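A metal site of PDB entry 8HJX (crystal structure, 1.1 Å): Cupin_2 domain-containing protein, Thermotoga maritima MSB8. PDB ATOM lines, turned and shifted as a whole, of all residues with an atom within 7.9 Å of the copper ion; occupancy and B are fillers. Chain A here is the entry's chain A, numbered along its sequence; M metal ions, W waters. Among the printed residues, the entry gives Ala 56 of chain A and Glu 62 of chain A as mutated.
Of the 20 residues printed, 3 come within 4 Å of the copper ion. The nearest printed residue that does not touch the copper ion is CSD 110 (5.3 Å).
O of His 96 is in hydrogen-bond range of N of Ala 56. The backbone carbonyl oxygen (O) of Glu 62 sits at hydrogen-bond distance from the backbone NH (N) of Val 90 (2.9 Å). The side-chain carboxylate (OE1) of Glu 62 lies close to OD1 of CSD 110 (2.5 Å). The backbone carbonyl oxygen of Glu 94 lies within hydrogen-bond range of a ring nitrogen (ND1) of His 96 (2.8 Å). The backbone carbonyl oxygen of Trp 60 lies within hydrogen-bond range of a ring nitrogen (ND1) of His 58.
Water W2 is bound to the copper ion (2.0 Å). NE2 of His 96 is bound to the copper ion, at 2.0 Å. The copper ion is bound by NE2 of His 58, 2.1 Å away. Water W1 binds the copper ion (2.2 Å). The copper ion is bound by OE2 of Glu 62 (2.3 Å).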
ATOM      1  N   ARG A  43      16.893  21.013  -9.958  1.00  0.00           N
ATOM      2  CA  ARG A  43      16.939  21.574 -11.289  1.00  0.00           C
ATOM      3  C   ARG A  43      16.492  23.034 -11.241  1.00  0.00           C
ATOM      4  O   ARG A  43      15.656  23.366 -10.365  1.00  0.00           O
ATOM      5  CB  ARG A  43      16.012  20.836 -12.268  1.00  0.00           C
ATOM      6  CG  ARG A  43      16.385  19.371 -12.431  1.00  0.00           C
ATOM      7  CD  ARG A  43      15.648  18.469 -11.476  1.00  0.00           C
ATOM      8  NE  ARG A  43      14.197  18.484 -11.571  1.00  0.00           N
ATOM      9  CZ  ARG A  43      13.436  17.889 -12.479  1.00  0.00           C
ATOM     10  NH1 ARG A  43      12.108  18.020 -12.401  1.00  0.00           N
ATOM     11  NH2 ARG A  43      14.008  17.187 -13.431  1.00  0.00           N
ATOM     12  N   PHE A  45      14.681  25.496 -13.882  1.00  0.00           N
ATOM     13  CA  PHE A  45      13.992  25.611 -15.151  1.00  0.00           C
ATOM     14  C   PHE A  45      13.829  27.063 -15.547  1.00  0.00           C
ATOM     15  O   PHE A  45      13.510  27.915 -14.699  1.00  0.00           O
ATOM     16  CB  PHE A  45      12.576  25.009 -15.075  1.00  0.00           C
ATOM     17  CG  PHE A  45      12.582  23.498 -15.156  1.00  0.00           C
ATOM     18  CD1 PHE A  45      12.254  22.889 -16.337  1.00  0.00           C
ATOM     19  CD2 PHE A  45      12.921  22.685 -14.098  1.00  0.00           C
ATOM     20  CE1 PHE A  45      12.241  21.525 -16.453  1.00  0.00           C
ATOM     21  CE2 PHE A  45      12.878  21.294 -14.205  1.00  0.00           C
ATOM     22  CZ  PHE A  45      12.550  20.715 -15.403  1.00  0.00           C
ATOM     23  N   ILE A  53       4.819  23.965 -20.455  1.00  0.00           N
ATOM     24  CA  ILE A  53       4.949  22.597 -19.927  1.00  0.00           C
ATOM     25  C   ILE A  53       3.523  22.130 -19.757  1.00  0.00           C
ATOM     26  O   ILE A  53       2.822  22.473 -18.809  1.00  0.00           O
ATOM     27  CB  ILE A  53       5.724  22.614 -18.622  1.00  0.00           C
ATOM     28  CG1 ILE A  53       7.146  23.194 -18.781  1.00  0.00           C
ATOM     29  CG2 ILE A  53       5.801  21.246 -17.960  1.00  0.00           C
ATOM     30  CD1 ILE A  53       7.794  23.610 -17.500  1.00  0.00           C
ATOM     31  N   ASP A  54       2.993  21.355 -20.708  1.00  0.00           N
ATOM     32  CA  ASP A  54       1.575  21.082 -20.722  1.00  0.00           C
ATOM     33  C   ASP A  54       1.197  20.141 -19.605  1.00  0.00           C
ATOM     34  O   ASP A  54       1.999  19.418 -19.065  1.00  0.00           O
ATOM     35  CB  ASP A  54       1.104  20.551 -22.087  1.00  0.00           C
ATOM     36  CG  ASP A  54      -0.331  20.951 -22.370  1.00  0.00           C
ATOM     37  OD1 ASP A  54      -0.994  21.652 -21.572  1.00  0.00           O
ATOM     38  OD2 ASP A  54      -0.856  20.465 -23.374  1.00  0.00           O
ATOM     39  N   ARG A  55      -0.093  20.163 -19.288  1.00  0.00           N
ATOM     40  CA  ARG A  55      -0.624  19.326 -18.221  1.00  0.00           C
ATOM     41  C   ARG A  55      -0.176  17.882 -18.368  1.00  0.00           C
ATOM     42  O   ARG A  55      -0.290  17.265 -19.434  1.00  0.00           O
ATOM     43  CB  ARG A  55      -2.139  19.369 -18.168  1.00  0.00           C
ATOM     44  CG  ARG A  55      -2.679  20.671 -17.595  1.00  0.00           C
ATOM     45  CD  ARG A  55      -4.211  20.658 -17.617  1.00  0.00           C
ATOM     46  NE  ARG A  55      -4.759  21.829 -17.015  1.00  0.00           N
ATOM     47  CZ  ARG A  55      -4.990  22.977 -17.606  1.00  0.00           C
ATOM     48  NH1 ARG A  55      -4.698  23.184 -18.887  1.00  0.00           N
ATOM     49  NH2 ARG A  55      -5.544  23.969 -16.900  1.00  0.00           N
ATOM     50  N   ALA A  56       0.257  17.312 -17.254  1.00  0.00           N
ATOM     51  CA  ALA A  56       0.721  15.955 -17.112  1.00  0.00           C
ATOM     52  C   ALA A  56       0.651  15.530 -15.676  1.00  0.00           C
ATOM     53  O   ALA A  56       0.411  16.334 -14.769  1.00  0.00           O
ATOM     54  CB  ALA A  56       2.164  15.846 -17.649  1.00  0.00           C
ATOM     55  N   SER A  57       0.913  14.240 -15.453  1.00  0.00           N
ATOM     56  CA  SER A  57       1.057  13.748 -14.120  1.00  0.00           C
ATOM     57  C   SER A  57       2.147  12.658 -14.159  1.00  0.00           C
ATOM     58  O   SER A  57       2.455  12.116 -15.199  1.00  0.00           O
ATOM     59  CB  SER A  57      -0.205  13.208 -13.516  1.00  0.00           C
ATOM     60  OG  SER A  57      -0.768  12.191 -14.275  1.00  0.00           O
ATOM     61  N   HIS A  58       2.667  12.374 -12.974  1.00  0.00           N
ATOM     62  CA  HIS A  58       3.711  11.367 -12.862  1.00  0.00           C
ATOM     63  C   HIS A  58       3.669  10.786 -11.463  1.00  0.00           C
ATOM     64  O   HIS A  58       3.175  11.425 -10.532  1.00  0.00           O
ATOM     65  CB  HIS A  58       5.105  11.874 -13.217  1.00  0.00           C
ATOM     66  CG  HIS A  58       5.347  13.243 -12.814  1.00  0.00           C
ATOM     67  ND1 HIS A  58       5.442  13.647 -11.494  1.00  0.00           N
ATOM     68  CD2 HIS A  58       5.563  14.342 -13.543  1.00  0.00           C
ATOM     69  CE1 HIS A  58       5.678  14.964 -11.479  1.00  0.00           C
ATOM     70  NE2 HIS A  58       5.767  15.428 -12.721  1.00  0.00           N
ATOM     71  N   TRP A  60       5.587  10.477  -8.951  1.00  0.00           N
ATOM     72  CA  TRP A  60       6.381  11.094  -7.914  1.00  0.00           C
ATOM     73  C   TRP A  60       5.851  12.511  -7.703  1.00  0.00           C
ATOM     74  O   TRP A  60       5.261  13.140  -8.599  1.00  0.00           O
ATOM     75  CB  TRP A  60       7.862  11.108  -8.270  1.00  0.00           C
ATOM     76  CG  TRP A  60       8.192  11.721  -9.586  1.00  0.00           C
ATOM     77  CD1 TRP A  60       8.398  13.045  -9.860  1.00  0.00           C
ATOM     78  CD2 TRP A  60       8.328  11.027 -10.839  1.00  0.00           C
ATOM     79  NE1 TRP A  60       8.669  13.201 -11.184  1.00  0.00           N
ATOM     80  CE2 TRP A  60       8.634  11.991 -11.818  1.00  0.00           C
ATOM     81  CE3 TRP A  60       8.225   9.679 -11.209  1.00  0.00           C
ATOM     82  CZ2 TRP A  60       8.840  11.633 -13.155  1.00  0.00           C
ATOM     83  CZ3 TRP A  60       8.435   9.348 -12.524  1.00  0.00           C
ATOM     84  CH2 TRP A  60       8.736  10.302 -13.473  1.00  0.00           C
ATOM     85  N   GLU A  61       6.151  13.030  -6.518  1.00  0.00           N
ATOM     86  CA  GLU A  61       5.871  14.398  -6.149  1.00  0.00           C
ATOM     87  C   GLU A  61       6.869  15.360  -6.755  1.00  0.00           C
ATOM     88  O   GLU A  61       7.946  14.970  -7.211  1.00  0.00           O
ATOM     89  CB  GLU A  61       5.927  14.568  -4.637  1.00  0.00           C
ATOM     90  CG  GLU A  61       7.295  14.507  -4.016  1.00  0.00           C
ATOM     91  CD  GLU A  61       7.898  13.154  -3.732  1.00  0.00           C
ATOM     92  OE1 GLU A  61       7.381  12.143  -4.283  1.00  0.00           O
ATOM     93  OE2 GLU A  61       8.901  13.123  -2.992  1.00  0.00           O
ATOM     94  N   GLU A  62       6.534  16.641  -6.722  1.00  0.00           N
ATOM     95  CA  GLU A  62       7.409  17.701  -7.179  1.00  0.00           C
ATOM     96  C   GLU A  62       7.338  18.848  -6.201  1.00  0.00           C
ATOM     97  O   GLU A  62       6.259  19.223  -5.736  1.00  0.00           O
ATOM     98  CB  GLU A  62       6.958  18.076  -8.582  1.00  0.00           C
ATOM     99  CG  GLU A  62       7.743  18.999  -9.408  1.00  0.00           C
ATOM    100  CD  GLU A  62       7.226  19.033 -10.838  1.00  0.00           C
ATOM    101  OE1 GLU A  62       7.540  20.030 -11.482  1.00  0.00           O
ATOM    102  OE2 GLU A  62       6.617  18.068 -11.337  1.00  0.00           O
ATOM    103  N   ILE A  64       8.557  22.905  -5.829  1.00  0.00           N
ATOM    104  CA  ILE A  64       8.978  24.010  -6.673  1.00  0.00           C
ATOM    105  C   ILE A  64       9.112  25.286  -5.838  1.00  0.00           C
ATOM    106  O   ILE A  64       8.321  25.518  -4.924  1.00  0.00           O
ATOM    107  CB  ILE A  64       7.945  24.220  -7.797  1.00  0.00           C
ATOM    108  CG1 ILE A  64       8.056  23.073  -8.808  1.00  0.00           C
ATOM    109  CG2 ILE A  64       8.065  25.526  -8.520  1.00  0.00           C
ATOM    110  CD1 ILE A  64       6.943  22.974  -9.825  1.00  0.00           C
ATOM    111  N   VAL A  90       3.399  19.586  -5.466  1.00  0.00           N
ATOM    112  CA  VAL A  90       2.534  18.804  -6.333  1.00  0.00           C
ATOM    113  C   VAL A  90       2.592  17.367  -5.847  1.00  0.00           C
ATOM    114  O   VAL A  90       3.651  16.732  -5.842  1.00  0.00           O
ATOM    115  CB  VAL A  90       3.027  18.852  -7.794  1.00  0.00           C
ATOM    116  CG1 VAL A  90       2.010  18.173  -8.700  1.00  0.00           C
ATOM    117  CG2 VAL A  90       3.250  20.267  -8.312  1.00  0.00           C
ATOM    118  N   GLU A  94      -0.821  14.106  -9.290  1.00  0.00           N
ATOM    119  CA  GLU A  94      -1.665  15.294  -9.480  1.00  0.00           C
ATOM    120  C   GLU A  94      -1.341  15.943 -10.802  1.00  0.00           C
ATOM    121  O   GLU A  94      -0.203  16.133 -11.189  1.00  0.00           O
ATOM    122  CB  GLU A  94      -1.397  16.237  -8.314  1.00  0.00           C
ATOM    123  CG  GLU A  94      -2.288  17.496  -8.364  1.00  0.00           C
ATOM    124  CD  GLU A  94      -3.729  17.154  -8.061  1.00  0.00           C
ATOM    125  OE1 GLU A  94      -4.666  17.834  -8.544  1.00  0.00           O
ATOM    126  OE2 GLU A  94      -4.046  16.206  -7.321  1.00  0.00           O
ATOM    127  N   ILE A  95      -2.390  16.294 -11.560  1.00  0.00           N
ATOM    128  CA  ILE A  95      -2.227  16.978 -12.797  1.00  0.00           C
ATOM    129  C   ILE A  95      -1.683  18.396 -12.603  1.00  0.00           C
ATOM    130  O   ILE A  95      -2.119  19.153 -11.695  1.00  0.00           O
ATOM    131  CB  ILE A  95      -3.561  17.061 -13.549  1.00  0.00           C
ATOM    132  CG1 ILE A  95      -4.022  15.689 -14.017  1.00  0.00           C
ATOM    133  CG2 ILE A  95      -3.536  18.065 -14.706  1.00  0.00           C
ATOM    134  CD1 ILE A  95      -5.501  15.536 -14.287  1.00  0.00           C
ATOM    135  N   HIS A  96      -0.707  18.764 -13.404  1.00  0.00           N
ATOM    136  CA  HIS A  96      -0.055  20.069 -13.248  1.00  0.00           C
ATOM    137  C   HIS A  96       0.635  20.393 -14.567  1.00  0.00           C
ATOM    138  O   HIS A  96       0.984  19.490 -15.341  1.00  0.00           O
ATOM    139  CB  HIS A  96       0.975  20.079 -12.113  1.00  0.00           C
ATOM    140  CG  HIS A  96       2.101  19.103 -12.356  1.00  0.00           C
ATOM    141  ND1 HIS A  96       1.894  17.750 -12.236  1.00  0.00           N
ATOM    142  CD2 HIS A  96       3.394  19.249 -12.717  1.00  0.00           C
ATOM    143  CE1 HIS A  96       3.035  17.114 -12.548  1.00  0.00           C
ATOM    144  NE2 HIS A  96       3.972  17.975 -12.827  1.00  0.00           N
ATOM    145  N   GLY A  97       0.852  21.659 -14.837  1.00  0.00           N
ATOM    146  CA  GLY A  97       1.658  22.139 -15.927  1.00  0.00           C
ATOM    147  C   GLY A  97       1.938  23.619 -15.698  1.00  0.00           C
ATOM    148  O   GLY A  97       1.514  24.160 -14.691  1.00  0.00           O
ATOM    149  N   PHE A  98       2.642  24.251 -16.626  1.00  0.00           N
ATOM    150  CA  PHE A  98       3.091  25.640 -16.418  1.00  0.00           C
ATOM    151  C   PHE A  98       3.129  26.365 -17.753  1.00  0.00           C
ATOM    152  O   PHE A  98       3.367  25.751 -18.794  1.00  0.00           O
ATOM    153  CB  PHE A  98       4.507  25.693 -15.840  1.00  0.00           C
ATOM    154  CG  PHE A  98       4.582  24.865 -14.594  1.00  0.00           C
ATOM    155  CD1 PHE A  98       4.149  25.384 -13.407  1.00  0.00           C
ATOM    156  CD2 PHE A  98       5.064  23.566 -14.639  1.00  0.00           C
ATOM    157  CE1 PHE A  98       4.170  24.606 -12.263  1.00  0.00           C
ATOM    158  CE2 PHE A  98       5.094  22.807 -13.484  1.00  0.00           C
ATOM    159  CZ  PHE A  98       4.646  23.297 -12.278  1.00  0.00           C
ATOM    160  N   CSD A 110      13.056  23.260  -9.221  1.00  0.00           N
ATOM    161  CA  CSD A 110      12.183  22.061  -9.220  1.00  0.00           C
ATOM    162  CB  CSD A 110      11.728  21.806 -10.651  1.00  0.00           C
ATOM    163  SG  CSD A 110      10.479  20.556 -10.587  1.00  0.00           S
ATOM    164  C   CSD A 110      13.013  20.902  -8.693  1.00  0.00           C
ATOM    165  O   CSD A 110      14.071  20.599  -9.220  1.00  0.00           O
ATOM    166  OD1 CSD A 110       9.887  20.495 -12.071  1.00  0.00           O
ATOM    167  OD2 CSD A 110      11.296  19.401 -10.502  1.00  0.00           O
ATOM    168  N   ILE A 112      12.685  16.783  -7.372  1.00  0.00           N
ATOM    169  CA  ILE A 112      11.940  15.558  -7.443  1.00  0.00           C
ATOM    170  C   ILE A 112      12.776  14.453  -6.801  1.00  0.00           C
ATOM    171  O   ILE A 112      14.014  14.536  -6.802  1.00  0.00           O
ATOM    172  CB  ILE A 112      11.523  15.149  -8.871  1.00  0.00           C
ATOM    173  CG1 ILE A 112      12.716  14.968  -9.790  1.00  0.00           C
ATOM    174  CG2 ILE A 112      10.519  16.142  -9.441  1.00  0.00           C
ATOM    175  CD1 ILE A 112      12.381  14.352 -11.132  1.00  0.00           C
HETATM  176 CU    CU M   1       5.805  17.403 -13.355  1.00  0.00          CU
HETATM  177  O   HOH W   1       6.252  19.225 -14.516  1.00  0.00           O
HETATM  178  O   HOH W   2       7.373  16.887 -14.412  1.00  0.00           O
